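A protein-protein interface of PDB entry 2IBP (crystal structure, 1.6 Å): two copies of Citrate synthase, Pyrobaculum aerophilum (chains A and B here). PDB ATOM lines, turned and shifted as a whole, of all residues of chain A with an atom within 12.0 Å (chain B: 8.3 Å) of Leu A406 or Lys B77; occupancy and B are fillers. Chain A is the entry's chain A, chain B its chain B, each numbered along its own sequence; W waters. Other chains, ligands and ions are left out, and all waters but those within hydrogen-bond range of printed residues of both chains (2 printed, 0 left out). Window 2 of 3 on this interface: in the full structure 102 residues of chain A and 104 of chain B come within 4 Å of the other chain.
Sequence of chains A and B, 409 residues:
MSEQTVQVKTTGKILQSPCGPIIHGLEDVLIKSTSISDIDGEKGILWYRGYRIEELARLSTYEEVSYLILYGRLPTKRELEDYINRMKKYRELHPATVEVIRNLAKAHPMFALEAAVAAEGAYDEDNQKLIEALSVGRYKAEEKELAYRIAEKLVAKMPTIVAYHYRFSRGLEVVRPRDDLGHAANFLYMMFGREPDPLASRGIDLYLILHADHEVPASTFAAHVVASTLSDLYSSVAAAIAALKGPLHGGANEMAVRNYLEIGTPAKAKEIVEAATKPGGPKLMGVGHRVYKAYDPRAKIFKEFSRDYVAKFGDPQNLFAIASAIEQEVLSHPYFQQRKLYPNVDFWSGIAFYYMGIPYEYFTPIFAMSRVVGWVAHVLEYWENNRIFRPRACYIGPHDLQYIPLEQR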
ATOM      1  N   GLN A 402     -10.792  -9.641  -8.703  1.00  0.00           N
ATOM      2  CA  GLN A 402     -10.874 -10.591  -9.793  1.00  0.00           C
ATOM      3  C   GLN A 402     -11.257  -9.914 -11.094  1.00  0.00           C
ATOM      4  O   GLN A 402     -12.321  -9.313 -11.189  1.00  0.00           O
ATOM      5  CB  GLN A 402     -11.928 -11.657  -9.460  1.00  0.00           C
ATOM      6  CG  GLN A 402     -12.261 -12.615 -10.605  1.00  0.00           C
ATOM      7  CD  GLN A 402     -11.062 -13.426 -11.066  1.00  0.00           C
ATOM      8  OE1 GLN A 402     -10.257 -13.891 -10.252  1.00  0.00           O
ATOM      9  NE2 GLN A 402     -10.955 -13.631 -12.376  1.00  0.00           N
ATOM     10  N   TYR A 403     -10.408 -10.056 -12.110  1.00  0.00           N
ATOM     11  CA  TYR A 403     -10.695  -9.531 -13.432  1.00  0.00           C
ATOM     12  C   TYR A 403     -11.922 -10.248 -13.991  1.00  0.00           C
ATOM     13  O   TYR A 403     -11.986 -11.477 -13.997  1.00  0.00           O
ATOM     14  CB  TYR A 403      -9.494  -9.748 -14.365  1.00  0.00           C
ATOM     15  CG  TYR A 403      -9.649  -9.133 -15.743  1.00  0.00           C
ATOM     16  CD1 TYR A 403      -9.146  -7.867 -16.028  1.00  0.00           C
ATOM     17  CD2 TYR A 403     -10.332  -9.795 -16.752  1.00  0.00           C
ATOM     18  CE1 TYR A 403      -9.321  -7.286 -17.279  1.00  0.00           C
ATOM     19  CE2 TYR A 403     -10.480  -9.238 -18.014  1.00  0.00           C
ATOM     20  CZ  TYR A 403      -9.968  -7.979 -18.269  1.00  0.00           C
ATOM     21  OH  TYR A 403     -10.129  -7.401 -19.505  1.00  0.00           O
ATOM     22  N   ILE A 404     -12.895  -9.466 -14.426  1.00  0.00           N
ATOM     23  CA  ILE A 404     -14.119  -9.983 -15.004  1.00  0.00           C
ATOM     24  C   ILE A 404     -14.098  -9.649 -16.484  1.00  0.00           C
ATOM     25  O   ILE A 404     -13.785  -8.525 -16.864  1.00  0.00           O
ATOM     26  CB  ILE A 404     -15.360  -9.364 -14.310  1.00  0.00           C
ATOM     27  CG1 ILE A 404     -15.468  -9.894 -12.876  1.00  0.00           C
ATOM     28  CG2 ILE A 404     -16.632  -9.683 -15.086  1.00  0.00           C
ATOM     29  CD1 ILE A 404     -16.630  -9.320 -12.092  1.00  0.00           C
ATOM     30  N   PRO A 405     -14.382 -10.637 -17.336  1.00  0.00           N
ATOM     31  CA  PRO A 405     -14.403 -10.373 -18.763  1.00  0.00           C
ATOM     32  C   PRO A 405     -15.332  -9.221 -19.111  1.00  0.00           C
ATOM     33  O   PRO A 405     -16.385  -9.068 -18.494  1.00  0.00           O
ATOM     34  CB  PRO A 405     -14.918 -11.691 -19.358  1.00  0.00           C
ATOM     35  CG  PRO A 405     -14.553 -12.707 -18.359  1.00  0.00           C
ATOM     36  CD  PRO A 405     -14.653 -12.053 -17.032  1.00  0.00           C
ATOM     37  N   LEU A 406     -14.944  -8.448 -20.121  1.00  0.00           N
ATOM     38  CA  LEU A 406     -15.680  -7.266 -20.541  1.00  0.00           C
ATOM     39  C   LEU A 406     -17.196  -7.450 -20.634  1.00  0.00           C
ATOM     40  O   LEU A 406     -17.956  -6.685 -20.035  1.00  0.00           O
ATOM     41  CB  LEU A 406     -15.149  -6.799 -21.894  1.00  0.00           C
ATOM     42  CG  LEU A 406     -15.670  -5.467 -22.415  1.00  0.00           C
ATOM     43  CD1 LEU A 406     -15.300  -4.320 -21.469  1.00  0.00           C
ATOM     44  CD2 LEU A 406     -15.104  -5.218 -23.809  1.00  0.00           C
ATOM     45  N   GLU A 407     -17.622  -8.475 -21.368  1.00  0.00           N
ATOM     46  CA  GLU A 407     -19.050  -8.711 -21.606  1.00  0.00           C
ATOM     47  C   GLU A 407     -19.876  -8.996 -20.354  1.00  0.00           C
ATOM     48  O   GLU A 407     -21.101  -8.896 -20.390  1.00  0.00           O
ATOM     49  CB  GLU A 407     -19.260  -9.837 -22.633  1.00  0.00           C
ATOM     50  CG  GLU A 407     -18.920 -11.254 -22.147  1.00  0.00           C
ATOM     51  CD  GLU A 407     -19.222 -12.331 -23.193  1.00  0.00           C
ATOM     52  OE1 GLU A 407     -19.654 -11.979 -24.314  1.00  0.00           O
ATOM     53  OE2 GLU A 407     -19.039 -13.533 -22.895  1.00  0.00           O
ATOM     54  N   GLN A 408     -19.221  -9.314 -19.243  1.00  0.00           N
ATOM     55  CA  GLN A 408     -19.935  -9.651 -18.012  1.00  0.00           C
ATOM     56  C   GLN A 408     -19.991  -8.522 -16.978  1.00  0.00           C
ATOM     57  O   GLN A 408     -20.502  -8.707 -15.876  1.00  0.00           O
ATOM     58  CB  GLN A 408     -19.311 -10.906 -17.407  1.00  0.00           C
ATOM     59  CG  GLN A 408     -19.296 -12.071 -18.398  1.00  0.00           C
ATOM     60  CD  GLN A 408     -18.524 -13.258 -17.894  1.00  0.00           C
ATOM     61  OE1 GLN A 408     -18.113 -14.117 -18.673  1.00  0.00           O
ATOM     62  NE2 GLN A 408     -18.305 -13.313 -16.578  1.00  0.00           N
ATOM     63  N   ARG A 409     -19.460  -7.353 -17.327  1.00  0.00           N
ATOM     64  CA  ARG A 409     -19.458  -6.219 -16.408  1.00  0.00           C
ATOM     65  C   ARG A 409     -20.716  -5.361 -16.524  1.00  0.00           C
ATOM     66  O   ARG A 409     -21.066  -4.645 -15.581  1.00  0.00           O
ATOM     67  CB  ARG A 409     -18.241  -5.345 -16.670  1.00  0.00           C
ATOM     68  CG  ARG A 409     -16.944  -6.087 -16.584  1.00  0.00           C
ATOM     69  CD  ARG A 409     -15.804  -5.167 -16.905  1.00  0.00           C
ATOM     70  NE  ARG A 409     -14.633  -5.961 -17.220  1.00  0.00           N
ATOM     71  CZ  ARG A 409     -13.622  -5.551 -17.974  1.00  0.00           C
ATOM     72  NH1 ARG A 409     -13.613  -4.337 -18.504  1.00  0.00           N
ATOM     73  NH2 ARG A 409     -12.648  -6.395 -18.237  1.00  0.00           N
ATOM     74  OXT ARG A 409     -21.369  -5.315 -17.570  1.00  0.00           O
ATOM     75  N   LEU B  59      -4.693 -10.172 -19.590  1.00  0.00           N
ATOM     76  CA  LEU B  59      -6.047 -10.065 -20.104  1.00  0.00           C
ATOM     77  C   LEU B  59      -6.488  -8.725 -20.638  1.00  0.00           C
ATOM     78  O   LEU B  59      -7.520  -8.639 -21.314  1.00  0.00           O
ATOM     79  CB  LEU B  59      -7.010 -10.477 -18.985  1.00  0.00           C
ATOM     80  CG  LEU B  59      -6.828 -11.900 -18.448  1.00  0.00           C
ATOM     81  CD1 LEU B  59      -7.674 -12.154 -17.204  1.00  0.00           C
ATOM     82  CD2 LEU B  59      -7.111 -12.962 -19.540  1.00  0.00           C
ATOM     83  N   GLU B  64      -7.808  -0.340 -21.827  1.00  0.00           N
ATOM     84  CA  GLU B  64      -8.558  -0.741 -20.646  1.00  0.00           C
ATOM     85  C   GLU B  64      -7.830  -0.427 -19.339  1.00  0.00           C
ATOM     86  O   GLU B  64      -8.438   0.016 -18.359  1.00  0.00           O
ATOM     87  CB  GLU B  64      -8.920  -2.215 -20.727  1.00  0.00           C
ATOM     88  CG  GLU B  64      -9.854  -2.656 -19.656  1.00  0.00           C
ATOM     89  CD  GLU B  64     -10.220  -4.125 -19.798  1.00  0.00           C
ATOM     90  OE1 GLU B  64      -9.326  -4.976 -19.642  1.00  0.00           O
ATOM     91  OE2 GLU B  64     -11.417  -4.417 -19.982  1.00  0.00           O
ATOM     92  N   ARG B  73     -11.883   1.785 -11.769  1.00  0.00           N
ATOM     93  CA  ARG B  73     -12.533   0.492 -11.939  1.00  0.00           C
ATOM     94  C   ARG B  73     -12.500   0.079 -13.391  1.00  0.00           C
ATOM     95  O   ARG B  73     -12.221   0.889 -14.277  1.00  0.00           O
ATOM     96  CB  ARG B  73     -13.982   0.558 -11.478  1.00  0.00           C
ATOM     97  CG  ARG B  73     -14.764   1.627 -12.174  1.00  0.00           C
ATOM     98  CD  ARG B  73     -16.221   1.578 -11.802  1.00  0.00           C
ATOM     99  NE  ARG B  73     -16.938   2.609 -12.529  1.00  0.00           N
ATOM    100  CZ  ARG B  73     -17.344   2.489 -13.788  1.00  0.00           C
ATOM    101  NH1 ARG B  73     -17.111   1.368 -14.470  1.00  0.00           N
ATOM    102  NH2 ARG B  73     -17.982   3.499 -14.360  1.00  0.00           N
ATOM    103  N   LEU B  74     -12.811  -1.189 -13.634  1.00  0.00           N
ATOM    104  CA  LEU B  74     -12.871  -1.691 -14.985  1.00  0.00           C
ATOM    105  C   LEU B  74     -14.099  -1.125 -15.689  1.00  0.00           C
ATOM    106  O   LEU B  74     -15.146  -0.933 -15.070  1.00  0.00           O
ATOM    107  CB  LEU B  74     -12.879  -3.224 -15.011  1.00  0.00           C
ATOM    108  CG  LEU B  74     -11.558  -3.890 -14.604  1.00  0.00           C
ATOM    109  CD1 LEU B  74     -11.787  -5.403 -14.457  1.00  0.00           C
ATOM    110  CD2 LEU B  74     -10.462  -3.607 -15.614  1.00  0.00           C
ATOM    111  N   PRO B  75     -13.960  -0.790 -16.975  1.00  0.00           N
ATOM    112  CA  PRO B  75     -15.098  -0.268 -17.697  1.00  0.00           C
ATOM    113  C   PRO B  75     -16.088  -1.339 -18.122  1.00  0.00           C
ATOM    114  O   PRO B  75     -15.718  -2.480 -18.373  1.00  0.00           O
ATOM    115  CB  PRO B  75     -14.466   0.327 -18.960  1.00  0.00           C
ATOM    116  CG  PRO B  75     -13.237  -0.493 -19.181  1.00  0.00           C
ATOM    117  CD  PRO B  75     -12.751  -0.875 -17.816  1.00  0.00           C
ATOM    118  N   THR B  76     -17.339  -0.943 -18.283  1.00  0.00           N
ATOM    119  CA  THR B  76     -18.298  -1.838 -18.880  1.00  0.00           C
ATOM    120  C   THR B  76     -17.972  -1.836 -20.370  1.00  0.00           C
ATOM    121  O   THR B  76     -17.187  -1.007 -20.850  1.00  0.00           O
ATOM    122  CB  THR B  76     -19.732  -1.323 -18.709  1.00  0.00           C
ATOM    123  OG1 THR B  76     -19.862  -0.063 -19.381  1.00  0.00           O
ATOM    124  CG2 THR B  76     -20.083  -1.179 -17.240  1.00  0.00           C
ATOM    125  N   LYS B  77     -18.611  -2.729 -21.113  1.00  0.00           N
ATOM    126  CA  LYS B  77     -18.410  -2.804 -22.549  1.00  0.00           C
ATOM    127  C   LYS B  77     -18.688  -1.446 -23.216  1.00  0.00           C
ATOM    128  O   LYS B  77     -17.884  -0.957 -24.023  1.00  0.00           O
ATOM    129  CB  LYS B  77     -19.307  -3.898 -23.134  1.00  0.00           C
ATOM    130  CG  LYS B  77     -19.262  -4.031 -24.651  1.00  0.00           C
ATOM    131  CD  LYS B  77     -20.162  -5.183 -25.094  1.00  0.00           C
ATOM    132  CE  LYS B  77     -20.338  -5.260 -26.606  1.00  0.00           C
ATOM    133  NZ  LYS B  77     -19.063  -5.541 -27.316  1.00  0.00           N
ATOM    134  N   ARG B  78     -19.826  -0.833 -22.884  1.00  0.00           N
ATOM    135  CA  ARG B  78     -20.181   0.468 -23.430  1.00  0.00           C
ATOM    136  C   ARG B  78     -19.191   1.570 -23.026  1.00  0.00           C
ATOM    137  O   ARG B  78     -18.822   2.412 -23.846  1.00  0.00           O
ATOM    138  CB  ARG B  78     -21.600   0.853 -23.003  1.00  0.00           C
ATOM    139  CG  ARG B  78     -22.055   2.223 -23.476  1.00  0.00           C
ATOM    140  CD  ARG B  78     -21.983   2.358 -24.991  1.00  0.00           C
ATOM    141  NE  ARG B  78     -22.472   3.660 -25.444  1.00  0.00           N
ATOM    142  CZ  ARG B  78     -22.448   4.071 -26.710  1.00  0.00           C
ATOM    143  NH1 ARG B  78     -21.933   3.294 -27.656  1.00  0.00           N
ATOM    144  NH2 ARG B  78     -22.913   5.275 -27.028  1.00  0.00           N
ATOM    145  N   GLU B  79     -18.782   1.572 -21.764  1.00  0.00           N
ATOM    146  CA  GLU B  79     -17.813   2.566 -21.284  1.00  0.00           C
ATOM    147  C   GLU B  79     -16.497   2.440 -22.019  1.00  0.00           C
ATOM    148  O   GLU B  79     -15.892   3.451 -22.387  1.00  0.00           O
ATOM    149  CB  GLU B  79     -17.565   2.406 -19.801  1.00  0.00           C
ATOM    150  CG  GLU B  79     -18.761   2.817 -18.978  1.00  0.00           C
ATOM    151  CD  GLU B  79     -18.597   2.528 -17.513  1.00  0.00           C
ATOM    152  OE1 GLU B  79     -17.851   1.588 -17.151  1.00  0.00           O
ATOM    153  OE2 GLU B  79     -19.253   3.230 -16.714  1.00  0.00           O
ATOM    154  N   LEU B  80     -16.049   1.208 -22.239  1.00  0.00           N
ATOM    155  CA  LEU B  80     -14.776   1.013 -22.945  1.00  0.00           C
ATOM    156  C   LEU B  80     -14.876   1.438 -24.404  1.00  0.00           C
ATOM    157  O   LEU B  80     -13.962   2.063 -24.942  1.00  0.00           O
ATOM    158  CB  LEU B  80     -14.290  -0.427 -22.845  1.00  0.00           C
ATOM    159  CG  LEU B  80     -12.898  -0.690 -23.425  1.00  0.00           C
ATOM    160  CD1 LEU B  80     -11.890   0.287 -22.816  1.00  0.00           C
ATOM    161  CD2 LEU B  80     -12.501  -2.133 -23.184  1.00  0.00           C
ATOM    162  N   GLU B  81     -15.973   1.080 -25.065  1.00  0.00           N
ATOM    163  CA  GLU B  81     -16.160   1.479 -26.450  1.00  0.00           C
ATOM    164  C   GLU B  81     -16.160   3.001 -26.602  1.00  0.00           C
ATOM    165  O   GLU B  81     -15.502   3.541 -27.496  1.00  0.00           O
ATOM    166  CB  GLU B  81     -17.470   0.911 -27.003  1.00  0.00           C
ATOM    167  CG  GLU B  81     -17.412  -0.581 -27.258  1.00  0.00           C
ATOM    168  CD  GLU B  81     -18.776  -1.205 -27.508  1.00  0.00           C
ATOM    169  OE1 GLU B  81     -19.808  -0.527 -27.299  1.00  0.00           O
ATOM    170  OE2 GLU B  81     -18.804  -2.392 -27.883  1.00  0.00           O
ATOM    171  N   ASP B  82     -16.928   3.679 -25.755  1.00  0.00           N
ATOM    172  CA  ASP B  82     -17.014   5.141 -25.803  1.00  0.00           C
ATOM    173  C   ASP B  82     -15.652   5.769 -25.505  1.00  0.00           C
ATOM    174  O   ASP B  82     -15.238   6.728 -26.163  1.00  0.00           O
ATOM    175  CB  ASP B  82     -18.057   5.646 -24.817  1.00  0.00           C
ATOM    176  CG  ASP B  82     -19.467   5.259 -25.228  1.00  0.00           C
ATOM    177  OD1 ASP B  82     -19.642   4.812 -26.387  1.00  0.00           O
ATOM    178  OD2 ASP B  82     -20.376   5.430 -24.400  1.00  0.00           O
ATOM    179  N   TYR B  83     -14.957   5.205 -24.525  1.00  0.00           N
ATOM    180  CA  TYR B  83     -13.628   5.699 -24.151  1.00  0.00           C
ATOM    181  C   TYR B  83     -12.647   5.559 -25.310  1.00  0.00           C
ATOM    182  O   TYR B  83     -11.916   6.494 -25.642  1.00  0.00           O
ATOM    183  CB  TYR B  83     -13.133   4.955 -22.923  1.00  0.00           C
ATOM    184  CG  TYR B  83     -11.716   5.266 -22.479  1.00  0.00           C
ATOM    185  CD1 TYR B  83     -11.436   6.405 -21.741  1.00  0.00           C
ATOM    186  CD2 TYR B  83     -10.704   4.340 -22.662  1.00  0.00           C
ATOM    187  CE1 TYR B  83     -10.160   6.636 -21.239  1.00  0.00           C
ATOM    188  CE2 TYR B  83      -9.418   4.592 -22.223  1.00  0.00           C
ATOM    189  CZ  TYR B  83      -9.148   5.737 -21.523  1.00  0.00           C
ATOM    190  OH  TYR B  83      -7.862   5.922 -21.033  1.00  0.00           O
ATOM    191  N   ILE B  84     -12.629   4.384 -25.924  1.00  0.00           N
ATOM    192  CA  ILE B  84     -11.739   4.132 -27.052  1.00  0.00           C
ATOM    193  C   ILE B  84     -12.005   5.111 -28.192  1.00  0.00           C
ATOM    194  O   ILE B  84     -11.081   5.660 -28.794  1.00  0.00           O
ATOM    195  CB  ILE B  84     -11.846   2.677 -27.503  1.00  0.00           C
ATOM    196  CG1 ILE B  84     -11.101   1.808 -26.481  1.00  0.00           C
ATOM    197  CG2 ILE B  84     -11.287   2.499 -28.898  1.00  0.00           C
ATOM    198  CD1 ILE B  84     -11.347   0.308 -26.649  1.00  0.00           C
HETATM  199  O   HOH W   1     -20.160  -4.933 -19.880  1.00  0.00           O
HETATM  200  O   HOH W   2     -11.420  -5.989 -22.277  1.00  0.00           O
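The guanidinium group (NH1) of Arg A409 sits at hydrogen-bond distance from the backbone carbonyl oxygen (O) of Pro B75.
O of Leu B59 lies within hydrogen-bond range of OH of Tyr A403 (3.4 Å).
NH1 of Arg A409 is in salt-bridge range of OE2 of Glu B64, at 2.6 Å.
The side-chain hydroxyl (OH) of Tyr A403 lies within hydrogen-bond range of the side-chain carboxylate (OE1) of Glu B64, at 2.6 Å.
Of the printed residues of chain B, Leu A406 touches Pro B75, Thr B76, Lys B77 and Leu B80.
Of chain A, only Leu A406 comes within 4 Å of Lys B77.
Of chain A, only Leu A406 (3.6 Å) and Arg A409 (2.8 Å) come within 4 Å of Pro B75.
Of the printed residues of chain A, Thr B76 touches Leu A406 (3.8 Å) and Arg A409 (3.97 Å).
Leu B80 touches one residue of chain A.
No residue of chain A comes within 4 Å of Glu B81.
Of the printed residues of chain A, Leu B59 touches Tyr A403.
Printed residues of chain B within 4 Å of Arg A409: Glu B64, Leu B74, Pro B75 and Thr B76.
Printed residues of chain A within 4 Å of Glu B64: Tyr A403 (2.6 Å) and Arg A409 (2.6 Å).
Printed residues of chain A within 4 Å of Leu B74: Tyr A403 (3.9 Å) and Arg A409 (3.7 Å).
Printed residues of chain B within 4 Å of Tyr A403: Leu B59 (3.4 Å), Glu B64 (2.6 Å) and Leu B74 (3.9 Å).
The nearest residue of chain B that does not touch Leu A406 is Glu B64 (4.2 Å).
The nearest residue of chain A that does not touch Lys B77 is Glu A407 (5.1 Å).
CD1 of Tyr A403 touches CD1 of Leu B74, at 3.9 Å.
Leu A406 touches Pro B75.
Thr B76 touches Leu A406 (C to CD1, 3.8 Å).
Leu A406 touches Lys B77 (CD1 to CA, 3.6 Å).
CD1 of Leu A406 touches CD2 of Leu B80, at 3.9 Å.
Leu B74 touches Arg A409.
Arg A409 touches Thr B76.
Among the printed residues, 11 pairs touch across the chains.
Among the printed residues, Asp or Glu carboxylates within 4 Å of a Lys or Arg side-chain nitrogen of the other chain: Arg A409 with Glu B64.
The backbone NH of Thr B76 sits at hydrogen-bond distance from the side-chain carboxylate of Glu B79 (2.8 Å).
O of Ile A404 is in hydrogen-bond range of NE of Arg A409 (2.7 Å).
NZ of Lys B77 is in salt-bridge range of OE2 of Glu B81.
OH of Tyr A403 is in hydrogen-bond range of NH2 of Arg A409.
Water W1 lies within hydrogen-bond range of the chain-end carboxylate of Arg A409 (2.6 Å), the backbone carbonyl oxygen of Leu A406 (2.8 Å) and the backbone NH of Lys B77 (3.0 Å).
Water W2 lies within hydrogen-bond range of OE2 of Glu B64 and OH of Tyr A403.
No position is printed for both chains.
Of the 11 pairs that touch across the chains among the printed residues, none has its exchanged pair printed and touching as well.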
